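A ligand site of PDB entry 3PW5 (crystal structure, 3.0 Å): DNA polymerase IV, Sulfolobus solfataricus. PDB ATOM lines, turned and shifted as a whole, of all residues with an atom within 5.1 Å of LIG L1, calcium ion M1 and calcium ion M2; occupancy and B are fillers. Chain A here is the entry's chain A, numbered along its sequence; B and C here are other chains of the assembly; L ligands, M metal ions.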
ATOM      1  N   ASP A  13      10.981 -16.573   4.147  1.00  0.00           N
ATOM      2  CA  ASP A  13      12.036 -17.561   4.269  1.00  0.00           C
ATOM      3  C   ASP A  13      12.401 -17.668   5.759  1.00  0.00           C
ATOM      4  O   ASP A  13      12.810 -16.678   6.356  1.00  0.00           O
ATOM      5  CB  ASP A  13      13.203 -17.047   3.465  1.00  0.00           C
ATOM      6  CG  ASP A  13      14.420 -17.853   3.644  1.00  0.00           C
ATOM      7  OD1 ASP A  13      14.394 -18.703   4.543  1.00  0.00           O
ATOM      8  OD2 ASP A  13      15.406 -17.631   2.912  1.00  0.00           O
ATOM      9  N   PHE A  14      12.264 -18.857   6.348  1.00  0.00           N
ATOM     10  CA  PHE A  14      12.538 -19.077   7.788  1.00  0.00           C
ATOM     11  C   PHE A  14      14.004 -19.118   8.167  1.00  0.00           C
ATOM     12  O   PHE A  14      14.757 -19.852   7.570  1.00  0.00           O
ATOM     13  CB  PHE A  14      11.926 -20.382   8.280  1.00  0.00           C
ATOM     14  CG  PHE A  14      10.620 -20.754   7.616  1.00  0.00           C
ATOM     15  CD1 PHE A  14       9.774 -19.788   7.111  1.00  0.00           C
ATOM     16  CD2 PHE A  14      10.244 -22.076   7.539  1.00  0.00           C
ATOM     17  CE1 PHE A  14       8.565 -20.142   6.549  1.00  0.00           C
ATOM     18  CE2 PHE A  14       9.029 -22.445   6.984  1.00  0.00           C
ATOM     19  CZ  PHE A  14       8.190 -21.473   6.483  1.00  0.00           C
ATOM     20  N   ASP A  15      14.391 -18.398   9.209  1.00  0.00           N
ATOM     21  CA  ASP A  15      15.807 -18.372   9.625  1.00  0.00           C
ATOM     22  C   ASP A  15      16.336 -19.681  10.192  1.00  0.00           C
ATOM     23  O   ASP A  15      15.650 -20.339  10.970  1.00  0.00           O
ATOM     24  CB  ASP A  15      16.027 -17.260  10.656  1.00  0.00           C
ATOM     25  CG  ASP A  15      15.502 -15.928  10.178  1.00  0.00           C
ATOM     26  OD1 ASP A  15      15.642 -15.629   8.961  1.00  0.00           O
ATOM     27  OD2 ASP A  15      14.968 -15.163  11.019  1.00  0.00           O
ATOM     28  N   TYR A  16      17.574 -20.032   9.830  1.00  0.00           N
ATOM     29  CA  TYR A  16      18.222 -21.271  10.279  1.00  0.00           C
ATOM     30  C   TYR A  16      17.199 -22.309  10.776  1.00  0.00           C
ATOM     31  O   TYR A  16      17.314 -22.845  11.854  1.00  0.00           O
ATOM     32  CB  TYR A  16      19.244 -20.953  11.375  1.00  0.00           C
ATOM     33  CG  TYR A  16      18.685 -20.304  12.629  1.00  0.00           C
ATOM     34  CD1 TYR A  16      18.210 -21.079  13.688  1.00  0.00           C
ATOM     35  CD2 TYR A  16      18.637 -18.908  12.774  1.00  0.00           C
ATOM     36  CE1 TYR A  16      17.726 -20.497  14.851  1.00  0.00           C
ATOM     37  CE2 TYR A  16      18.159 -18.311  13.931  1.00  0.00           C
ATOM     38  CZ  TYR A  16      17.707 -19.114  14.976  1.00  0.00           C
ATOM     39  OH  TYR A  16      17.216 -18.566  16.131  1.00  0.00           O
ATOM     40  N   PHE A  17      16.211 -22.576   9.925  1.00  0.00           N
ATOM     41  CA  PHE A  17      15.083 -23.479  10.189  1.00  0.00           C
ATOM     42  C   PHE A  17      15.197 -24.752  11.030  1.00  0.00           C
ATOM     43  O   PHE A  17      14.502 -24.870  12.026  1.00  0.00           O
ATOM     44  CB  PHE A  17      14.403 -23.830   8.869  1.00  0.00           C
ATOM     45  CG  PHE A  17      13.056 -24.477   9.034  1.00  0.00           C
ATOM     46  CD1 PHE A  17      12.020 -23.794   9.643  1.00  0.00           C
ATOM     47  CD2 PHE A  17      12.840 -25.768   8.609  1.00  0.00           C
ATOM     48  CE1 PHE A  17      10.791 -24.392   9.843  1.00  0.00           C
ATOM     49  CE2 PHE A  17      11.605 -26.377   8.792  1.00  0.00           C
ATOM     50  CZ  PHE A  17      10.575 -25.683   9.418  1.00  0.00           C
ATOM     51  N   TYR A  18      16.022 -25.724  10.631  1.00  0.00           N
ATOM     52  CA  TYR A  18      16.135 -26.948  11.429  1.00  0.00           C
ATOM     53  C   TYR A  18      16.667 -26.586  12.798  1.00  0.00           C
ATOM     54  O   TYR A  18      16.083 -26.957  13.799  1.00  0.00           O
ATOM     55  CB  TYR A  18      17.108 -27.951  10.822  1.00  0.00           C
ATOM     56  CG  TYR A  18      16.622 -28.656   9.596  1.00  0.00           C
ATOM     57  CD1 TYR A  18      15.481 -28.254   8.934  1.00  0.00           C
ATOM     58  CD2 TYR A  18      17.371 -29.707   9.065  1.00  0.00           C
ATOM     59  CE1 TYR A  18      15.079 -28.876   7.762  1.00  0.00           C
ATOM     60  CE2 TYR A  18      16.992 -30.337   7.895  1.00  0.00           C
ATOM     61  CZ  TYR A  18      15.847 -29.922   7.243  1.00  0.00           C
ATOM     62  OH  TYR A  18      15.486 -30.539   6.075  1.00  0.00           O
ATOM     63  N   VAL A  49      27.226 -31.262   8.289  1.00  0.00           N
ATOM     64  CA  VAL A  49      26.368 -30.403   9.085  1.00  0.00           C
ATOM     65  C   VAL A  49      25.174 -29.966   8.236  1.00  0.00           C
ATOM     66  O   VAL A  49      25.357 -29.341   7.184  1.00  0.00           O
ATOM     67  CB  VAL A  49      27.141 -29.142   9.571  1.00  0.00           C
ATOM     68  CG1 VAL A  49      26.187 -28.120  10.192  1.00  0.00           C
ATOM     69  CG2 VAL A  49      28.215 -29.534  10.575  1.00  0.00           C
ATOM     70  N   ALA A  50      23.961 -30.297   8.673  1.00  0.00           N
ATOM     71  CA  ALA A  50      22.754 -29.900   7.955  1.00  0.00           C
ATOM     72  C   ALA A  50      22.621 -28.384   8.071  1.00  0.00           C
ATOM     73  O   ALA A  50      22.374 -27.693   7.082  1.00  0.00           O
ATOM     74  CB  ALA A  50      21.540 -30.567   8.541  1.00  0.00           C
ATOM     75  N   THR A  51      22.785 -27.860   9.279  1.00  0.00           N
ATOM     76  CA  THR A  51      22.719 -26.420   9.514  1.00  0.00           C
ATOM     77  C   THR A  51      23.086 -26.032  10.934  1.00  0.00           C
ATOM     78  O   THR A  51      23.180 -26.889  11.814  1.00  0.00           O
ATOM     79  CB  THR A  51      21.313 -25.832   9.194  1.00  0.00           C
ATOM     80  OG1 THR A  51      21.329 -24.420   9.467  1.00  0.00           O
ATOM     81  CG2 THR A  51      20.243 -26.490  10.045  1.00  0.00           C
ATOM     82  N   ALA A  52      23.299 -24.740  11.153  1.00  0.00           N
ATOM     83  CA  ALA A  52      23.658 -24.252  12.473  1.00  0.00           C
ATOM     84  C   ALA A  52      22.989 -22.920  12.719  1.00  0.00           C
ATOM     85  O   ALA A  52      22.881 -22.109  11.812  1.00  0.00           O
ATOM     86  CB  ALA A  52      25.162 -24.096  12.565  1.00  0.00           C
ATOM     87  N   TYR A  54      22.713 -19.085  14.284  1.00  0.00           N
ATOM     88  CA  TYR A  54      23.715 -18.039  14.136  1.00  0.00           C
ATOM     89  C   TYR A  54      24.834 -17.963  15.157  1.00  0.00           C
ATOM     90  O   TYR A  54      25.928 -17.504  14.850  1.00  0.00           O
ATOM     91  CB  TYR A  54      23.014 -16.682  14.016  1.00  0.00           C
ATOM     92  CG  TYR A  54      22.326 -16.538  12.680  1.00  0.00           C
ATOM     93  CD1 TYR A  54      23.043 -16.185  11.535  1.00  0.00           C
ATOM     94  CD2 TYR A  54      20.974 -16.828  12.550  1.00  0.00           C
ATOM     95  CE1 TYR A  54      22.421 -16.136  10.303  1.00  0.00           C
ATOM     96  CE2 TYR A  54      20.346 -16.785  11.313  1.00  0.00           C
ATOM     97  CZ  TYR A  54      21.076 -16.438  10.200  1.00  0.00           C
ATOM     98  OH  TYR A  54      20.442 -16.419   8.981  1.00  0.00           O
ATOM     99  N   ARG A  57      27.263 -20.178  13.874  1.00  0.00           N
ATOM    100  CA  ARG A  57      27.611 -19.712  12.549  1.00  0.00           C
ATOM    101  C   ARG A  57      28.582 -18.516  12.555  1.00  0.00           C
ATOM    102  O   ARG A  57      29.240 -18.232  11.556  1.00  0.00           O
ATOM    103  CB  ARG A  57      26.320 -19.387  11.803  1.00  0.00           C
ATOM    104  CG  ARG A  57      26.509 -19.098  10.351  1.00  0.00           C
ATOM    105  CD  ARG A  57      25.196 -18.742   9.739  1.00  0.00           C
ATOM    106  NE  ARG A  57      24.234 -19.813   9.911  1.00  0.00           N
ATOM    107  CZ  ARG A  57      23.252 -20.066   9.054  1.00  0.00           C
ATOM    108  NH1 ARG A  57      23.118 -19.309   7.979  1.00  0.00           N
ATOM    109  NH2 ARG A  57      22.420 -21.081   9.257  1.00  0.00           N
ATOM    110  N   ALA A  63      26.532 -24.966   7.257  1.00  0.00           N
ATOM    111  CA  ALA A  63      26.065 -26.190   6.603  1.00  0.00           C
ATOM    112  C   ALA A  63      27.035 -26.738   5.571  1.00  0.00           C
ATOM    113  O   ALA A  63      27.510 -26.020   4.711  1.00  0.00           O
ATOM    114  CB  ALA A  63      24.702 -25.976   5.952  1.00  0.00           C
ATOM    115  N   GLY A  64      27.320 -28.033   5.679  1.00  0.00           N
ATOM    116  CA  GLY A  64      28.217 -28.657   4.733  1.00  0.00           C
ATOM    117  C   GLY A  64      29.573 -29.064   5.295  1.00  0.00           C
ATOM    118  O   GLY A  64      30.087 -30.121   4.946  1.00  0.00           O
ATOM    119  N   MET A  82      19.639 -34.691  13.040  1.00  0.00           N
ATOM    120  CA  MET A  82      18.523 -34.101  12.309  1.00  0.00           C
ATOM    121  C   MET A  82      17.278 -34.998  12.257  1.00  0.00           C
ATOM    122  O   MET A  82      17.364 -36.187  11.959  1.00  0.00           O
ATOM    123  CB  MET A  82      18.991 -33.746  10.894  1.00  0.00           C
ATOM    124  CG  MET A  82      17.914 -33.193  10.016  1.00  0.00           C
ATOM    125  SD  MET A  82      18.205 -33.650   8.309  1.00  0.00           S
ATOM    126  CE  MET A  82      18.283 -35.467   8.407  1.00  0.00           C
ATOM    127  N   SER A 109      10.443 -24.448  -1.098  1.00  0.00           N
ATOM    128  CA  SER A 109      11.094 -25.522  -0.349  1.00  0.00           C
ATOM    129  C   SER A 109      10.452 -25.742   1.007  1.00  0.00           C
ATOM    130  O   SER A 109       9.350 -25.292   1.254  1.00  0.00           O
ATOM    131  CB  SER A 109      12.570 -25.208  -0.158  1.00  0.00           C
ATOM    132  OG  SER A 109      12.734 -24.169   0.790  1.00  0.00           O
ATOM    133  N   ILE A 110      11.174 -26.430   1.887  1.00  0.00           N
ATOM    134  CA  ILE A 110      10.645 -26.697   3.202  1.00  0.00           C
ATOM    135  C   ILE A 110      10.653 -25.438   4.039  1.00  0.00           C
ATOM    136  O   ILE A 110      10.103 -25.401   5.127  1.00  0.00           O
ATOM    137  CB  ILE A 110      11.468 -27.813   3.914  1.00  0.00           C
ATOM    138  CG1 ILE A 110      10.699 -28.318   5.138  1.00  0.00           C
ATOM    139  CG2 ILE A 110      12.862 -27.311   4.254  1.00  0.00           C
ATOM    140  CD1 ILE A 110      11.254 -29.588   5.726  1.00  0.00           C
ATOM    141  N   ASP A 111      11.229 -24.369   3.506  1.00  0.00           N
ATOM    142  CA  ASP A 111      11.268 -23.128   4.265  1.00  0.00           C
ATOM    143  C   ASP A 111      11.066 -21.872   3.414  1.00  0.00           C
ATOM    144  O   ASP A 111      11.162 -20.764   3.941  1.00  0.00           O
ATOM    145  CB  ASP A 111      12.605 -23.010   4.953  1.00  0.00           C
ATOM    146  CG  ASP A 111      13.676 -22.628   3.985  1.00  0.00           C
ATOM    147  OD1 ASP A 111      14.419 -23.498   3.497  1.00  0.00           O
ATOM    148  OD2 ASP A 111      13.751 -21.430   3.692  1.00  0.00           O
ATOM    149  N   GLU A 112      10.826 -22.026   2.130  1.00  0.00           N
ATOM    150  CA  GLU A 112      10.668 -20.861   1.259  1.00  0.00           C
ATOM    151  C   GLU A 112       9.355 -20.882   0.539  1.00  0.00           C
ATOM    152  O   GLU A 112       8.954 -21.910   0.002  1.00  0.00           O
ATOM    153  CB  GLU A 112      11.799 -20.821   0.227  1.00  0.00           C
ATOM    154  CG  GLU A 112      13.194 -20.798   0.820  1.00  0.00           C
ATOM    155  CD  GLU A 112      14.301 -21.223  -0.155  1.00  0.00           C
ATOM    156  OE1 GLU A 112      14.468 -20.556  -1.200  1.00  0.00           O
ATOM    157  OE2 GLU A 112      15.023 -22.213   0.146  1.00  0.00           O
ATOM    158  N   LYS A 165      18.780 -10.945   6.175  1.00  0.00           N
ATOM    159  CA  LYS A 165      18.831 -12.093   7.098  1.00  0.00           C
ATOM    160  C   LYS A 165      19.606 -11.743   8.361  1.00  0.00           C
ATOM    161  O   LYS A 165      20.668 -11.104   8.296  1.00  0.00           O
ATOM    162  CB  LYS A 165      19.496 -13.317   6.442  1.00  0.00           C
ATOM    163  CG  LYS A 165      18.720 -14.002   5.329  1.00  0.00           C
ATOM    164  CD  LYS A 165      19.407 -15.308   4.942  1.00  0.00           C
ATOM    165  CE  LYS A 165      18.982 -15.806   3.553  1.00  0.00           C
ATOM    166  NZ  LYS A 165      17.519 -16.037   3.382  1.00  0.00           N
ATOM    167  P    DT B   2      22.741 -41.268   5.610  1.00  0.00           P
ATOM    168  OP1  DT B   2      23.060 -42.238   4.542  1.00  0.00           O
ATOM    169  OP2  DT B   2      23.822 -40.452   6.206  1.00  0.00           O
ATOM    170  O5'  DT B   2      21.605 -40.289   5.060  1.00  0.00           O
ATOM    171  C5'  DT B   2      21.589 -38.910   5.416  1.00  0.00           C
ATOM    172  C4'  DT B   2      20.206 -38.329   5.243  1.00  0.00           C
ATOM    173  O4'  DT B   2      20.200 -36.952   5.714  1.00  0.00           O
ATOM    174  C3'  DT B   2      19.716 -38.181   3.797  1.00  0.00           C
ATOM    175  O3'  DT B   2      18.291 -38.255   3.767  1.00  0.00           O
ATOM    176  C2'  DT B   2      20.164 -36.840   3.383  1.00  0.00           C
ATOM    177  C1'  DT B   2      19.954 -36.043   4.644  1.00  0.00           C
ATOM    178  N1   DT B   2      20.896 -34.918   4.803  1.00  0.00           N
ATOM    179  C2   DT B   2      20.390 -33.650   4.968  1.00  0.00           C
ATOM    180  O2   DT B   2      19.189 -33.398   5.017  1.00  0.00           O
ATOM    181  N3   DT B   2      21.350 -32.666   5.060  1.00  0.00           N
ATOM    182  C4   DT B   2      22.725 -32.828   5.005  1.00  0.00           C
ATOM    183  O4   DT B   2      23.470 -31.852   5.088  1.00  0.00           O
ATOM    184  C5   DT B   2      23.183 -34.196   4.844  1.00  0.00           C
ATOM    185  C7   DT B   2      24.650 -34.470   4.798  1.00  0.00           C
ATOM    186  C6   DT B   2      22.247 -35.152   4.747  1.00  0.00           C
ATOM    187  P    DC C  13      21.847 -21.124  -6.291  1.00  0.00           P
ATOM    188  OP1  DC C  13      21.543 -19.713  -6.613  1.00  0.00           O
ATOM    189  OP2  DC C  13      23.193 -21.519  -5.818  1.00  0.00           O
ATOM    190  O5'  DC C  13      20.826 -21.586  -5.179  1.00  0.00           O
ATOM    191  C5'  DC C  13      19.421 -21.486  -5.379  1.00  0.00           C
ATOM    192  C4'  DC C  13      18.716 -22.271  -4.305  1.00  0.00           C
ATOM    193  O4'  DC C  13      18.986 -23.678  -4.510  1.00  0.00           O
ATOM    194  C3'  DC C  13      19.265 -21.986  -2.899  1.00  0.00           C
ATOM    195  O3'  DC C  13      18.287 -21.868  -1.853  1.00  0.00           O
ATOM    196  C2'  DC C  13      20.151 -23.138  -2.595  1.00  0.00           C
ATOM    197  C1'  DC C  13      19.452 -24.261  -3.316  1.00  0.00           C
ATOM    198  N1   DC C  13      20.306 -25.407  -3.646  1.00  0.00           N
ATOM    199  C2   DC C  13      19.763 -26.702  -3.588  1.00  0.00           C
ATOM    200  O2   DC C  13      18.544 -26.845  -3.372  1.00  0.00           O
ATOM    201  N3   DC C  13      20.578 -27.769  -3.765  1.00  0.00           N
ATOM    202  C4   DC C  13      21.872 -27.587  -4.024  1.00  0.00           C
ATOM    203  N4   DC C  13      22.631 -28.666  -4.154  1.00  0.00           N
ATOM    204  C5   DC C  13      22.435 -26.289  -4.152  1.00  0.00           C
ATOM    205  C6   DC C  13      21.625 -25.238  -3.961  1.00  0.00           C
HETATM  206  P1  LIG L   1      18.361 -22.499   4.153  1.00  0.00           P
HETATM  207  O1  LIG L   1      16.854 -22.725   4.303  1.00  0.00           O
HETATM  208  O2  LIG L   1      18.703 -22.157   2.749  1.00  0.00           O
HETATM  209  O3  LIG L   1      18.647 -21.267   5.026  1.00  0.00           O
HETATM  210  P2  LIG L   1      18.482 -21.226   6.619  1.00  0.00           P
HETATM  211  O4  LIG L   1      18.084 -22.441   7.346  1.00  0.00           O
HETATM  212  O5  LIG L   1      17.507 -20.155   6.847  1.00  0.00           O
HETATM  213  O6  LIG L   1      19.835 -20.653   6.917  1.00  0.00           O
HETATM  214  P3  LIG L   1      20.082 -19.230   7.319  1.00  0.00           P
HETATM  215  O7  LIG L   1      20.998 -18.548   6.383  1.00  0.00           O
HETATM  216  O8  LIG L   1      18.743 -18.384   7.389  1.00  0.00           O
HETATM  217  O9  LIG L   1      20.601 -19.239   8.837  1.00  0.00           O
HETATM  218  O10 LIG L   1      19.028 -23.743   4.939  1.00  0.00           O
HETATM  219  C1  LIG L   1      18.501 -24.796   4.701  1.00  0.00           C
HETATM  220  C2  LIG L   1      17.452 -25.565   5.419  1.00  0.00           C
HETATM  221  O11 LIG L   1      17.579 -26.614   4.384  1.00  0.00           O
HETATM  222  C3  LIG L   1      17.961 -25.998   6.757  1.00  0.00           C
HETATM  223  O12 LIG L   1      17.170 -25.824   7.679  1.00  0.00           O
HETATM  224  C4  LIG L   1      18.409 -27.421   6.535  1.00  0.00           C
HETATM  225  C5  LIG L   1      18.260 -27.699   5.006  1.00  0.00           C
HETATM  226  N1  LIG L   1      19.737 -28.050   4.548  1.00  0.00           N
HETATM  227  C6  LIG L   1      20.325 -29.300   4.692  1.00  0.00           C
HETATM  228  O13 LIG L   1      19.749 -30.250   5.193  1.00  0.00           O
HETATM  229  N2  LIG L   1      21.650 -29.394   4.215  1.00  0.00           N
HETATM  230  C7  LIG L   1      22.414 -28.387   3.629  1.00  0.00           C
HETATM  231  O14 LIG L   1      23.579 -28.605   3.247  1.00  0.00           O
HETATM  232  C8  LIG L   1      21.724 -27.110   3.517  1.00  0.00           C
HETATM  233  C9  LIG L   1      22.490 -25.924   2.883  1.00  0.00           C
HETATM  234  C10 LIG L   1      20.462 -26.992   3.967  1.00  0.00           C
HETATM  235  C1  LG2 L   2      22.181 -33.873  -1.390  1.00  0.00           C
HETATM  236  C2  LG2 L   2      23.128 -32.696  -0.993  1.00  0.00           C
HETATM  237  O1  LG2 L   2      24.480 -32.989  -1.285  1.00  0.00           O
HETATM  238  C3  LG2 L   2      22.940 -32.502   0.532  1.00  0.00           C
HETATM  239  C4  LG2 L   2      21.700 -31.712   0.924  1.00  0.00           C
HETATM  240  O2  LG2 L   2      22.495 -34.734  -0.222  1.00  0.00           O
HETATM  241  C5  LG2 L   2      22.562 -33.934   1.017  1.00  0.00           C
HETATM  242  O3  LG2 L   2      21.261 -33.864   1.664  1.00  0.00           O
HETATM  243  C6  LG2 L   2      20.808 -32.565   1.554  1.00  0.00           C
HETATM  244  C7  LG2 L   2      19.534 -32.114   1.978  1.00  0.00           C
HETATM  245  C8  LG2 L   2      19.141 -30.750   1.747  1.00  0.00           C
HETATM  246  O4  LG2 L   2      17.888 -30.295   2.138  1.00  0.00           O
HETATM  247  C9  LG2 L   2      16.866 -31.055   2.790  1.00  0.00           C
HETATM  248  C10 LG2 L   2      20.102 -29.826   1.063  1.00  0.00           C
HETATM  249  C11 LG2 L   2      21.393 -30.368   0.676  1.00  0.00           C
HETATM  250  O5  LG2 L   2      22.335 -29.563   0.025  1.00  0.00           O
HETATM  251  C12 LG2 L   2      22.118 -28.190  -0.294  1.00  0.00           C
HETATM  252  O6  LG2 L   2      23.037 -27.591  -0.854  1.00  0.00           O
HETATM  253  C13 LG2 L   2      20.832 -27.647   0.086  1.00  0.00           C
HETATM  254  C14 LG2 L   2      19.872 -28.443   0.726  1.00  0.00           C
HETATM  255  C15 LG2 L   2      18.639 -27.614   0.996  1.00  0.00           C
HETATM  256  C16 LG2 L   2      18.967 -26.235   0.435  1.00  0.00           C
HETATM  257  C17 LG2 L   2      20.380 -26.324  -0.140  1.00  0.00           C
HETATM  258  O7  LG2 L   2      20.932 -25.363  -0.667  1.00  0.00           O
HETATM  259 CA    CA M   1      15.651 -20.379   5.396  1.00  0.00          CA
HETATM  260 CA    CA M   2      15.955 -20.645   2.255  1.00  0.00          CA
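The backbone NH (N) of Tyr 18 sits at hydrogen-bond distance from an oxygen (O12) of LIG L1 (3.2 Å). The guanidinium group (NH2) of Arg 57 is in salt-bridge range of an oxygen (O9) of LIG L1. An oxygen (O8) of LIG L1 is in hydrogen-bond range of the backbone NH of Tyr 16. A nitrogen (N2) of LIG L1 lies within hydrogen-bond range of O4 of DT 2 of chain B. N of Phe 17 sits at hydrogen-bond distance from O4 of LIG L1 (3.2 Å). A nitrogen (N2) of LIG L1 lies within hydrogen-bond range of the backbone carbonyl oxygen (O) of Ala 50 (3.4 Å). The side-chain hydroxyl (OH) of Tyr 54 is in hydrogen-bond range of an oxygen (O9) of LIG L1, at 2.8 Å.
The side-chain hydroxyl of Ser 109 lies close to the backbone NH of Asp 111. NZ of Lys 165 lies within salt-bridge range of OD2 of Asp 13 of chain A (2.7 Å). The guanidinium group (NH2) of Arg 57 sits at hydrogen-bond distance from the backbone carbonyl oxygen (O) of Ala 52 (2.8 Å). N of Glu 112 sits at hydrogen-bond distance from OG of Ser 109 (3.2 Å).
C of Asp 15 touches O5 of LIG L1, 3.6 Å away. CG2 of Thr 51 touches O12 of LIG L1, at 3.9 Å. Ala 63 touches LIG L1. CD of Lys 165 touches O7 of LIG L1, 3.9 Å away. 13 residues have an atom within 4 Å of LIG L1: Phe 14, Asp 15, Tyr 16, Phe 17, Tyr 18, Ala 50, Thr 51, Tyr 54, Arg 57, Ala 63, Asp 111, Lys 165 and DT 2 of chain B. The nearest printed residue that does not touch LIG L1 is Asp 13 of chain A (4.1 Å).
Three residues have an atom within 4 Å of calcium ion M1: Asp 13 of chain A, Phe 14 and Asp 111.
Three residues have an atom within 4 Å of calcium ion M2: Asp 13 of chain A, Asp 111 and Glu 112.
Calcium ion M1 is bound by the side-chain carboxylate (OD1) of Asp 13 of chain A (2.3 Å), an oxygen (O5) of LIG L1 (2.4 Å), the backbone carbonyl oxygen (O) of Phe 14 (2.4 Å), the side-chain carboxylate (OD2) of Asp 111 (2.8 Å) and an oxygen (O1) of LIG L1 (2.9 Å). Calcium ion M1 has five donor atoms within binding distance. Slightly farther from calcium ion M1 lies O3 of LIG L1 (3.1 Å).
Calcium ion M2 is bound by OD2 of Asp 111, 2.7 Å away. The side-chain carboxylate (OE2) of Glu 112 binds calcium ion M2, 2.8 Å away. Slightly farther from calcium ion M2 lies an oxygen (O1) of LIG L1 (3.1 Å). Slightly farther from calcium ion M2 lies the side-chain carboxylate (OD2) of Asp 13 of chain A (3.1 Å).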
